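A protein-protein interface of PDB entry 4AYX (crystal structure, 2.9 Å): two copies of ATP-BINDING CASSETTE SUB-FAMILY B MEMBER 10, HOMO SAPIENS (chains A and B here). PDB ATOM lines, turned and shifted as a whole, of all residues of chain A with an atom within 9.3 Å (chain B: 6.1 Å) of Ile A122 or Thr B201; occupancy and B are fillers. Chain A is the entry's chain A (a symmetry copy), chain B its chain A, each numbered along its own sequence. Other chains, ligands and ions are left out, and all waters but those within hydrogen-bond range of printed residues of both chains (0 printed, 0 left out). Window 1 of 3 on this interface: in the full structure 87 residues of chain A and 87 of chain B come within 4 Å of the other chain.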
ATOM      1  N   ARG A  98      25.924 -17.978  25.869  1.00  0.00           N
ATOM      2  CA  ARG A  98      25.554 -17.068  24.783  1.00  0.00           C
ATOM      3  C   ARG A  98      25.177 -17.836  23.494  1.00  0.00           C
ATOM      4  O   ARG A  98      24.080 -17.637  22.960  1.00  0.00           O
ATOM      5  CB  ARG A  98      26.695 -16.086  24.493  1.00  0.00           C
ATOM      6  CG  ARG A  98      26.705 -14.863  25.383  1.00  0.00           C
ATOM      7  CD  ARG A  98      28.011 -14.136  25.192  1.00  0.00           C
ATOM      8  NE  ARG A  98      28.153 -12.996  26.093  1.00  0.00           N
ATOM      9  CZ  ARG A  98      29.315 -12.581  26.590  1.00  0.00           C
ATOM     10  NH1 ARG A  98      30.438 -13.227  26.302  1.00  0.00           N
ATOM     11  NH2 ARG A  98      29.356 -11.539  27.411  1.00  0.00           N
ATOM     12  N   LEU A 101      22.039 -20.128  24.067  1.00  0.00           N
ATOM     13  CA  LEU A 101      20.795 -19.376  24.197  1.00  0.00           C
ATOM     14  C   LEU A 101      20.344 -18.808  22.848  1.00  0.00           C
ATOM     15  O   LEU A 101      19.164 -18.930  22.530  1.00  0.00           O
ATOM     16  CB  LEU A 101      20.914 -18.254  25.255  1.00  0.00           C
ATOM     17  CG  LEU A 101      19.633 -17.452  25.562  1.00  0.00           C
ATOM     18  CD1 LEU A 101      18.681 -18.237  26.449  1.00  0.00           C
ATOM     19  CD2 LEU A 101      19.961 -16.130  26.189  1.00  0.00           C
ATOM     20  N   PHE A 102      21.263 -18.189  22.065  1.00  0.00           N
ATOM     21  CA  PHE A 102      20.951 -17.600  20.756  1.00  0.00           C
ATOM     22  C   PHE A 102      20.442 -18.664  19.771  1.00  0.00           C
ATOM     23  O   PHE A 102      19.503 -18.395  19.015  1.00  0.00           O
ATOM     24  CB  PHE A 102      22.160 -16.862  20.183  1.00  0.00           C
ATOM     25  CG  PHE A 102      21.806 -15.994  19.003  1.00  0.00           C
ATOM     26  CD1 PHE A 102      20.950 -14.908  19.149  1.00  0.00           C
ATOM     27  CD2 PHE A 102      22.298 -16.282  17.737  1.00  0.00           C
ATOM     28  CE1 PHE A 102      20.598 -14.124  18.049  1.00  0.00           C
ATOM     29  CE2 PHE A 102      21.962 -15.485  16.640  1.00  0.00           C
ATOM     30  CZ  PHE A 102      21.109 -14.414  16.801  1.00  0.00           C
ATOM     31  N   ILE A 105      16.856 -19.519  20.787  1.00  0.00           N
ATOM     32  CA  ILE A 105      15.959 -18.427  20.421  1.00  0.00           C
ATOM     33  C   ILE A 105      15.579 -18.543  18.936  1.00  0.00           C
ATOM     34  O   ILE A 105      14.387 -18.660  18.637  1.00  0.00           O
ATOM     35  CB  ILE A 105      16.537 -17.018  20.768  1.00  0.00           C
ATOM     36  CG1 ILE A 105      16.663 -16.807  22.279  1.00  0.00           C
ATOM     37  CG2 ILE A 105      15.677 -15.897  20.156  1.00  0.00           C
ATOM     38  CD1 ILE A 105      17.636 -15.656  22.679  1.00  0.00           C
ATOM     39  N   PHE A 113       7.942 -15.162  19.369  1.00  0.00           N
ATOM     40  CA  PHE A 113       8.481 -13.816  19.207  1.00  0.00           C
ATOM     41  C   PHE A 113       7.363 -12.791  19.269  1.00  0.00           C
ATOM     42  O   PHE A 113       7.615 -11.645  19.634  1.00  0.00           O
ATOM     43  CB  PHE A 113       9.269 -13.696  17.885  1.00  0.00           C
ATOM     44  CG  PHE A 113      10.505 -14.562  17.848  1.00  0.00           C
ATOM     45  CD1 PHE A 113      10.437 -15.879  17.406  1.00  0.00           C
ATOM     46  CD2 PHE A 113      11.730 -14.071  18.261  1.00  0.00           C
ATOM     47  CE1 PHE A 113      11.571 -16.694  17.410  1.00  0.00           C
ATOM     48  CE2 PHE A 113      12.867 -14.877  18.228  1.00  0.00           C
ATOM     49  CZ  PHE A 113      12.779 -16.183  17.809  1.00  0.00           C
ATOM     50  N   THR A 116       7.001 -12.382  23.028  1.00  0.00           N
ATOM     51  CA  THR A 116       8.224 -12.041  23.750  1.00  0.00           C
ATOM     52  C   THR A 116       8.931 -10.868  23.079  1.00  0.00           C
ATOM     53  O   THR A 116       9.300 -10.950  21.902  1.00  0.00           O
ATOM     54  CB  THR A 116       9.143 -13.249  23.859  1.00  0.00           C
ATOM     55  OG1 THR A 116       8.366 -14.408  24.153  1.00  0.00           O
ATOM     56  CG2 THR A 116      10.242 -13.053  24.890  1.00  0.00           C
ATOM     57  N   ARG A 117       9.143  -9.785  23.850  1.00  0.00           N
ATOM     58  CA  ARG A 117       9.824  -8.564  23.402  1.00  0.00           C
ATOM     59  C   ARG A 117      11.305  -8.846  23.200  1.00  0.00           C
ATOM     60  O   ARG A 117      11.880  -9.603  23.985  1.00  0.00           O
ATOM     61  CB  ARG A 117       9.623  -7.420  24.412  1.00  0.00           C
ATOM     62  CG  ARG A 117       8.166  -6.996  24.599  1.00  0.00           C
ATOM     63  CD  ARG A 117       8.026  -5.598  25.193  1.00  0.00           C
ATOM     64  NE  ARG A 117       8.356  -4.537  24.230  1.00  0.00           N
ATOM     65  CZ  ARG A 117       7.495  -3.994  23.372  1.00  0.00           C
ATOM     66  NH1 ARG A 117       6.234  -4.412  23.330  1.00  0.00           N
ATOM     67  NH2 ARG A 117       7.892  -3.038  22.542  1.00  0.00           N
ATOM     68  N   THR A 118      11.913  -8.267  22.135  1.00  0.00           N
ATOM     69  CA  THR A 118      13.329  -8.446  21.768  1.00  0.00           C
ATOM     70  C   THR A 118      14.230  -7.952  22.911  1.00  0.00           C
ATOM     71  O   THR A 118      15.239  -8.601  23.210  1.00  0.00           O
ATOM     72  CB  THR A 118      13.634  -7.749  20.429  1.00  0.00           C
ATOM     73  OG1 THR A 118      12.717  -8.227  19.452  1.00  0.00           O
ATOM     74  CG2 THR A 118      15.063  -7.972  19.944  1.00  0.00           C
ATOM     75  N   GLY A 119      13.828  -6.847  23.553  1.00  0.00           N
ATOM     76  CA  GLY A 119      14.522  -6.263  24.698  1.00  0.00           C
ATOM     77  C   GLY A 119      14.743  -7.251  25.827  1.00  0.00           C
ATOM     78  O   GLY A 119      15.843  -7.308  26.378  1.00  0.00           O
ATOM     79  N   GLU A 120      13.716  -8.069  26.149  1.00  0.00           N
ATOM     80  CA  GLU A 120      13.804  -9.096  27.182  1.00  0.00           C
ATOM     81  C   GLU A 120      14.775 -10.202  26.755  1.00  0.00           C
ATOM     82  O   GLU A 120      15.578 -10.657  27.576  1.00  0.00           O
ATOM     83  CB  GLU A 120      12.415  -9.684  27.505  1.00  0.00           C
ATOM     84  CG  GLU A 120      12.374 -10.651  28.689  1.00  0.00           C
ATOM     85  CD  GLU A 120      13.024 -10.189  29.985  1.00  0.00           C
ATOM     86  OE1 GLU A 120      12.690  -9.078  30.460  1.00  0.00           O
ATOM     87  OE2 GLU A 120      13.887 -10.932  30.513  1.00  0.00           O
ATOM     88  N   LEU A 121      14.726 -10.610  25.474  1.00  0.00           N
ATOM     89  CA  LEU A 121      15.595 -11.667  24.948  1.00  0.00           C
ATOM     90  C   LEU A 121      17.060 -11.217  24.947  1.00  0.00           C
ATOM     91  O   LEU A 121      17.929 -11.998  25.334  1.00  0.00           O
ATOM     92  CB  LEU A 121      15.141 -12.119  23.552  1.00  0.00           C
ATOM     93  CG  LEU A 121      13.781 -12.838  23.506  1.00  0.00           C
ATOM     94  CD1 LEU A 121      13.282 -13.004  22.078  1.00  0.00           C
ATOM     95  CD2 LEU A 121      13.841 -14.182  24.202  1.00  0.00           C
ATOM     96  N   ILE A 122      17.316  -9.938  24.603  1.00  0.00           N
ATOM     97  CA  ILE A 122      18.652  -9.340  24.615  1.00  0.00           C
ATOM     98  C   ILE A 122      19.124  -9.168  26.077  1.00  0.00           C
ATOM     99  O   ILE A 122      20.274  -9.508  26.371  1.00  0.00           O
ATOM    100  CB  ILE A 122      18.681  -8.027  23.791  1.00  0.00           C
ATOM    101  CG1 ILE A 122      18.524  -8.323  22.273  1.00  0.00           C
ATOM    102  CG2 ILE A 122      19.929  -7.170  24.075  1.00  0.00           C
ATOM    103  CD1 ILE A 122      19.502  -9.435  21.680  1.00  0.00           C
ATOM    104  N   ASN A 123      18.230  -8.743  26.997  1.00  0.00           N
ATOM    105  CA  ASN A 123      18.586  -8.625  28.419  1.00  0.00           C
ATOM    106  C   ASN A 123      18.971  -9.989  28.982  1.00  0.00           C
ATOM    107  O   ASN A 123      19.959 -10.079  29.705  1.00  0.00           O
ATOM    108  CB  ASN A 123      17.465  -7.987  29.264  1.00  0.00           C
ATOM    109  CG  ASN A 123      17.483  -6.470  29.320  1.00  0.00           C
ATOM    110  OD1 ASN A 123      18.528  -5.809  29.178  1.00  0.00           O
ATOM    111  ND2 ASN A 123      16.320  -5.888  29.583  1.00  0.00           N
ATOM    112  N   ARG A 124      18.246 -11.050  28.595  1.00  0.00           N
ATOM    113  CA  ARG A 124      18.559 -12.422  29.016  1.00  0.00           C
ATOM    114  C   ARG A 124      19.873 -12.895  28.382  1.00  0.00           C
ATOM    115  O   ARG A 124      20.579 -13.699  28.973  1.00  0.00           O
ATOM    116  CB  ARG A 124      17.414 -13.390  28.658  1.00  0.00           C
ATOM    117  CG  ARG A 124      16.205 -13.246  29.564  1.00  0.00           C
ATOM    118  CD  ARG A 124      15.147 -14.284  29.295  1.00  0.00           C
ATOM    119  NE  ARG A 124      13.869 -13.888  29.898  1.00  0.00           N
ATOM    120  CZ  ARG A 124      12.927 -14.734  30.316  1.00  0.00           C
ATOM    121  NH1 ARG A 124      13.110 -16.045  30.220  1.00  0.00           N
ATOM    122  NH2 ARG A 124      11.801 -14.272  30.846  1.00  0.00           N
ATOM    123  N   LEU A 125      20.206 -12.378  27.186  1.00  0.00           N
ATOM    124  CA  LEU A 125      21.413 -12.767  26.463  1.00  0.00           C
ATOM    125  C   LEU A 125      22.628 -12.014  26.965  1.00  0.00           C
ATOM    126  O   LEU A 125      23.736 -12.564  26.961  1.00  0.00           O
ATOM    127  CB  LEU A 125      21.235 -12.558  24.947  1.00  0.00           C
ATOM    128  CG  LEU A 125      22.355 -13.068  24.020  1.00  0.00           C
ATOM    129  CD1 LEU A 125      22.427 -14.590  23.995  1.00  0.00           C
ATOM    130  CD2 LEU A 125      22.169 -12.543  22.628  1.00  0.00           C
ATOM    131  N   SER A 126      22.432 -10.764  27.394  1.00  0.00           N
ATOM    132  CA  SER A 126      23.542  -9.944  27.854  1.00  0.00           C
ATOM    133  C   SER A 126      23.711 -10.000  29.381  1.00  0.00           C
ATOM    134  O   SER A 126      24.724 -10.515  29.872  1.00  0.00           O
ATOM    135  CB  SER A 126      23.365  -8.507  27.379  1.00  0.00           C
ATOM    136  OG  SER A 126      22.072  -8.036  27.723  1.00  0.00           O
ATOM    137  N   SER A 127      22.708  -9.503  30.116  1.00  0.00           N
ATOM    138  CA  SER A 127      22.751  -9.389  31.566  1.00  0.00           C
ATOM    139  C   SER A 127      22.728 -10.736  32.281  1.00  0.00           C
ATOM    140  O   SER A 127      23.651 -11.022  33.057  1.00  0.00           O
ATOM    141  CB  SER A 127      21.608  -8.513  32.067  1.00  0.00           C
ATOM    142  OG  SER A 127      21.408  -7.389  31.220  1.00  0.00           O
ATOM    143  N   ASP A 128      21.691 -11.554  32.032  1.00  0.00           N
ATOM    144  CA  ASP A 128      21.488 -12.812  32.750  1.00  0.00           C
ATOM    145  C   ASP A 128      22.574 -13.866  32.503  1.00  0.00           C
ATOM    146  O   ASP A 128      22.823 -14.683  33.395  1.00  0.00           O
ATOM    147  CB  ASP A 128      20.098 -13.389  32.463  1.00  0.00           C
ATOM    148  CG  ASP A 128      18.944 -12.551  33.003  1.00  0.00           C
ATOM    149  OD1 ASP A 128      19.170 -11.747  33.947  1.00  0.00           O
ATOM    150  OD2 ASP A 128      17.813 -12.708  32.499  1.00  0.00           O
ATOM    151  N   THR A 129      23.234 -13.839  31.331  1.00  0.00           N
ATOM    152  CA  THR A 129      24.317 -14.777  31.018  1.00  0.00           C
ATOM    153  C   THR A 129      25.563 -14.378  31.810  1.00  0.00           C
ATOM    154  O   THR A 129      26.310 -15.255  32.242  1.00  0.00           O
ATOM    155  CB  THR A 129      24.595 -14.851  29.506  1.00  0.00           C
ATOM    156  OG1 THR A 129      24.954 -13.561  29.011  1.00  0.00           O
ATOM    157  CG2 THR A 129      23.426 -15.412  28.719  1.00  0.00           C
ATOM    158  N   ALA A 130      25.767 -13.053  32.015  1.00  0.00           N
ATOM    159  CA  ALA A 130      26.899 -12.504  32.768  1.00  0.00           C
ATOM    160  C   ALA A 130      26.752 -12.826  34.241  1.00  0.00           C
ATOM    161  O   ALA A 130      27.731 -13.227  34.872  1.00  0.00           O
ATOM    162  CB  ALA A 130      27.006 -11.002  32.561  1.00  0.00           C
ATOM    163  N   LEU A 315      16.981 -18.415  31.982  1.00  0.00           N
ATOM    164  CA  LEU A 315      17.797 -18.976  30.909  1.00  0.00           C
ATOM    165  C   LEU A 315      17.449 -20.428  30.644  1.00  0.00           C
ATOM    166  O   LEU A 315      17.247 -20.777  29.483  1.00  0.00           O
ATOM    167  CB  LEU A 315      19.289 -18.820  31.210  1.00  0.00           C
ATOM    168  CG  LEU A 315      19.794 -17.378  31.159  1.00  0.00           C
ATOM    169  CD1 LEU A 315      21.032 -17.202  31.985  1.00  0.00           C
ATOM    170  CD2 LEU A 315      20.074 -16.950  29.762  1.00  0.00           C
ATOM    171  N   LEU A 318      14.374 -20.848  28.411  1.00  0.00           N
ATOM    172  CA  LEU A 318      14.519 -20.729  26.966  1.00  0.00           C
ATOM    173  C   LEU A 318      15.388 -21.843  26.400  1.00  0.00           C
ATOM    174  O   LEU A 318      15.115 -22.326  25.293  1.00  0.00           O
ATOM    175  CB  LEU A 318      15.115 -19.369  26.573  1.00  0.00           C
ATOM    176  CG  LEU A 318      14.327 -18.102  26.904  1.00  0.00           C
ATOM    177  CD1 LEU A 318      15.118 -16.876  26.532  1.00  0.00           C
ATOM    178  CD2 LEU A 318      12.984 -18.061  26.185  1.00  0.00           C
ATOM    179  N   LYS A 480      21.741   0.646  11.092  1.00  0.00           N
ATOM    180  CA  LYS A 480      22.995   1.182  11.630  1.00  0.00           C
ATOM    181  C   LYS A 480      23.952   1.727  10.533  1.00  0.00           C
ATOM    182  O   LYS A 480      24.985   2.317  10.868  1.00  0.00           O
ATOM    183  CB  LYS A 480      23.715   0.120  12.497  1.00  0.00           C
ATOM    184  CG  LYS A 480      22.873  -0.488  13.634  1.00  0.00           C
ATOM    185  CD  LYS A 480      22.479   0.507  14.745  1.00  0.00           C
ATOM    186  CE  LYS A 480      20.992   0.795  14.795  1.00  0.00           C
ATOM    187  NZ  LYS A 480      20.212  -0.340  15.360  1.00  0.00           N
ATOM    188  N   SER B 196      33.644  -5.178  20.751  1.00  0.00           N
ATOM    189  CA  SER B 196      33.452  -6.468  20.102  1.00  0.00           C
ATOM    190  C   SER B 196      32.157  -7.120  20.589  1.00  0.00           C
ATOM    191  O   SER B 196      31.381  -7.608  19.763  1.00  0.00           O
ATOM    192  CB  SER B 196      34.639  -7.373  20.398  1.00  0.00           C
ATOM    193  OG  SER B 196      34.851  -8.291  19.343  1.00  0.00           O
ATOM    194  N   LEU B 197      31.910  -7.090  21.920  1.00  0.00           N
ATOM    195  CA  LEU B 197      30.708  -7.640  22.541  1.00  0.00           C
ATOM    196  C   LEU B 197      29.465  -6.856  22.109  1.00  0.00           C
ATOM    197  O   LEU B 197      28.417  -7.472  21.882  1.00  0.00           O
ATOM    198  CB  LEU B 197      30.838  -7.660  24.078  1.00  0.00           C
ATOM    199  CG  LEU B 197      29.646  -8.218  24.876  1.00  0.00           C
ATOM    200  CD1 LEU B 197      29.344  -9.662  24.507  1.00  0.00           C
ATOM    201  CD2 LEU B 197      29.869  -8.079  26.357  1.00  0.00           C
ATOM    202  N   ALA B 198      29.586  -5.513  21.982  1.00  0.00           N
ATOM    203  CA  ALA B 198      28.499  -4.635  21.549  1.00  0.00           C
ATOM    204  C   ALA B 198      28.043  -4.997  20.132  1.00  0.00           C
ATOM    205  O   ALA B 198      26.834  -5.106  19.894  1.00  0.00           O
ATOM    206  CB  ALA B 198      28.946  -3.186  21.606  1.00  0.00           C
ATOM    207  N   GLN B 199      29.025  -5.215  19.210  1.00  0.00           N
ATOM    208  CA  GLN B 199      28.819  -5.609  17.809  1.00  0.00           C
ATOM    209  C   GLN B 199      27.990  -6.900  17.722  1.00  0.00           C
ATOM    210  O   GLN B 199      26.997  -6.947  16.990  1.00  0.00           O
ATOM    211  CB  GLN B 199      30.171  -5.819  17.102  1.00  0.00           C
ATOM    212  CG  GLN B 199      30.880  -4.545  16.649  1.00  0.00           C
ATOM    213  CD  GLN B 199      31.972  -4.841  15.636  1.00  0.00           C
ATOM    214  OE1 GLN B 199      32.789  -5.762  15.794  1.00  0.00           O
ATOM    215  NE2 GLN B 199      32.013  -4.062  14.566  1.00  0.00           N
ATOM    216  N   ALA B 200      28.398  -7.929  18.508  1.00  0.00           N
ATOM    217  CA  ALA B 200      27.757  -9.236  18.600  1.00  0.00           C
ATOM    218  C   ALA B 200      26.318  -9.121  19.121  1.00  0.00           C
ATOM    219  O   ALA B 200      25.445  -9.859  18.659  1.00  0.00           O
ATOM    220  CB  ALA B 200      28.572 -10.156  19.499  1.00  0.00           C
ATOM    221  N   THR B 201      26.064  -8.194  20.064  1.00  0.00           N
ATOM    222  CA  THR B 201      24.728  -8.025  20.644  1.00  0.00           C
ATOM    223  C   THR B 201      23.827  -7.267  19.658  1.00  0.00           C
ATOM    224  O   THR B 201      22.632  -7.574  19.573  1.00  0.00           O
ATOM    225  CB  THR B 201      24.798  -7.389  22.041  1.00  0.00           C
ATOM    226  OG1 THR B 201      25.633  -8.208  22.868  1.00  0.00           O
ATOM    227  CG2 THR B 201      23.425  -7.278  22.695  1.00  0.00           C
ATOM    228  N   GLN B 202      24.401  -6.325  18.881  1.00  0.00           N
ATOM    229  CA  GLN B 202      23.640  -5.600  17.861  1.00  0.00           C
ATOM    230  C   GLN B 202      23.195  -6.579  16.780  1.00  0.00           C
ATOM    231  O   GLN B 202      22.028  -6.541  16.374  1.00  0.00           O
ATOM    232  CB  GLN B 202      24.439  -4.429  17.262  1.00  0.00           C
ATOM    233  CG  GLN B 202      23.581  -3.459  16.412  1.00  0.00           C
ATOM    234  CD  GLN B 202      22.333  -2.954  17.119  1.00  0.00           C
ATOM    235  OE1 GLN B 202      22.398  -2.244  18.131  1.00  0.00           O
ATOM    236  NE2 GLN B 202      21.164  -3.323  16.604  1.00  0.00           N
ATOM    237  N   LEU B 203      24.099  -7.496  16.375  1.00  0.00           N
ATOM    238  CA  LEU B 203      23.814  -8.561  15.417  1.00  0.00           C
ATOM    239  C   LEU B 203      22.650  -9.415  15.936  1.00  0.00           C
ATOM    240  O   LEU B 203      21.659  -9.585  15.229  1.00  0.00           O
ATOM    241  CB  LEU B 203      25.072  -9.416  15.195  1.00  0.00           C
ATOM    242  CG  LEU B 203      24.901 -10.725  14.439  1.00  0.00           C
ATOM    243  CD1 LEU B 203      24.842 -10.495  12.955  1.00  0.00           C
ATOM    244  CD2 LEU B 203      26.022 -11.656  14.750  1.00  0.00           C
ATOM    245  N   ALA B 204      22.749  -9.868  17.199  1.00  0.00           N
ATOM    246  CA  ALA B 204      21.756 -10.674  17.898  1.00  0.00           C
ATOM    247  C   ALA B 204      20.384  -9.985  17.910  1.00  0.00           C
ATOM    248  O   ALA B 204      19.401 -10.591  17.480  1.00  0.00           O
ATOM    249  CB  ALA B 204      22.230 -10.944  19.313  1.00  0.00           C
ATOM    250  N   GLU B 205      20.339  -8.701  18.341  1.00  0.00           N
ATOM    251  CA  GLU B 205      19.143  -7.856  18.407  1.00  0.00           C
ATOM    252  C   GLU B 205      18.501  -7.676  17.041  1.00  0.00           C
ATOM    253  O   GLU B 205      17.272  -7.767  16.940  1.00  0.00           O
ATOM    254  CB  GLU B 205      19.511  -6.488  18.987  1.00  0.00           C
ATOM    255  CG  GLU B 205      18.329  -5.583  19.276  1.00  0.00           C
ATOM    256  CD  GLU B 205      18.680  -4.244  19.893  1.00  0.00           C
ATOM    257  OE1 GLU B 205      19.803  -3.739  19.653  1.00  0.00           O
ATOM    258  OE2 GLU B 205      17.806  -3.685  20.597  1.00  0.00           O
ATOM    259  N   GLU B 206      19.326  -7.413  15.997  1.00  0.00           N
ATOM    260  CA  GLU B 206      18.854  -7.216  14.625  1.00  0.00           C
ATOM    261  C   GLU B 206      18.207  -8.488  14.086  1.00  0.00           C
ATOM    262  O   GLU B 206      17.101  -8.414  13.563  1.00  0.00           O
ATOM    263  CB  GLU B 206      20.001  -6.764  13.705  1.00  0.00           C
ATOM    264  CG  GLU B 206      19.553  -6.349  12.306  1.00  0.00           C
ATOM    265  CD  GLU B 206      20.586  -5.567  11.520  1.00  0.00           C
ATOM    266  OE1 GLU B 206      21.712  -6.081  11.332  1.00  0.00           O
ATOM    267  OE2 GLU B 206      20.266  -4.437  11.083  1.00  0.00           O
ATOM    268  N   ILE B 208      17.120 -11.247  15.864  1.00  0.00           N
ATOM    269  CA  ILE B 208      15.952 -11.617  16.685  1.00  0.00           C
ATOM    270  C   ILE B 208      14.746 -10.746  16.277  1.00  0.00           C
ATOM    271  O   ILE B 208      13.656 -11.277  16.049  1.00  0.00           O
ATOM    272  CB  ILE B 208      16.245 -11.545  18.220  1.00  0.00           C
ATOM    273  CG1 ILE B 208      17.203 -12.675  18.641  1.00  0.00           C
ATOM    274  CG2 ILE B 208      14.944 -11.608  19.057  1.00  0.00           C
ATOM    275  CD1 ILE B 208      17.908 -12.407  19.918  1.00  0.00           C
ATOM    276  N   TYR B 227      26.972 -15.535  14.793  1.00  0.00           N
ATOM    277  CA  TYR B 227      26.988 -15.017  16.154  1.00  0.00           C
ATOM    278  C   TYR B 227      27.991 -15.798  16.997  1.00  0.00           C
ATOM    279  O   TYR B 227      28.787 -15.174  17.698  1.00  0.00           O
ATOM    280  CB  TYR B 227      25.586 -15.069  16.772  1.00  0.00           C
ATOM    281  CG  TYR B 227      25.543 -14.661  18.228  1.00  0.00           C
ATOM    282  CD1 TYR B 227      25.493 -13.317  18.595  1.00  0.00           C
ATOM    283  CD2 TYR B 227      25.533 -15.618  19.241  1.00  0.00           C
ATOM    284  CE1 TYR B 227      25.456 -12.935  19.936  1.00  0.00           C
ATOM    285  CE2 TYR B 227      25.499 -15.248  20.584  1.00  0.00           C
ATOM    286  CZ  TYR B 227      25.450 -13.906  20.927  1.00  0.00           C
ATOM    287  OH  TYR B 227      25.408 -13.552  22.251  1.00  0.00           O
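NH2 of Arg A98 touches CD1 of Leu B197, 3.5 Å away. Arg A98 touches Tyr B227 (CB to OH, 3.6 Å). Phe A102 touches Ala B204 (CE1 to CA, 3.6 Å). Phe A102 touches Tyr B227 (CD2 to CD2, 3.6 Å). CG2 of Thr A118 touches O of Glu B205, at 3.7 Å. Ile B208 touches Thr A118. Leu A121 touches Ile B208 (CD1 to CG2, 3.7 Å). Ile A122 touches Thr B201. Ile A122 touches Ala B204. CD1 of Ile A122 touches N of Glu B205, 3.5 Å away.
Of the 13 printed residues of chain B, 7 touch a printed residue of chain A. Of the 23 printed residues of chain A, 9 touch a printed residue of chain B. Hydrophobic or aromatic side chains of chain A that line the printed part of chain B: Phe A102, Ile A105, Phe A113, Leu A121, Ile A122 and Leu A125.
The backbone carbonyl oxygen of Leu B197 sits at hydrogen-bond distance from the side-chain hydroxyl of Thr B201, at 3.0 Å. OE1 of Glu B205 lies close to OE1 of Gln B202 (3.4 Å). OG of Ser A126 sits at hydrogen-bond distance from O of Ile A122 (2.7 Å). The side-chain hydroxyl of Thr A129 lies within hydrogen-bond range of the backbone carbonyl oxygen of Leu A125, at 2.6 Å.
NE2 of Gln B202 lies close to NZ of Lys A480 (3.4 Å).
Glu A120 touches none of the printed residues of chain B. Ile A122 touches just these residues of chain B: Thr B201, Ala B204, Glu B205 and Ile B208. Printed residues of chain A within 4 Å of Leu B197: Arg A98. Of chain A, only Ile A122 comes within 4 Å of Thr B201. Of chain A, only Phe A102 (3.6 Å), Ile A122 (3.9 Å) and Leu A125 (3.7 Å) come within 4 Å of Ala B204. Of the printed residues of chain A, Glu B205 touches Thr A118 and Ile A122. The nearest residue of chain A that does not touch Thr B201 is Ser A126 (4.8 Å). The nearest printed residue of chain B that does not touch Phe A113 is Ala B204 (7.8 Å).
No position is printed for both chains.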
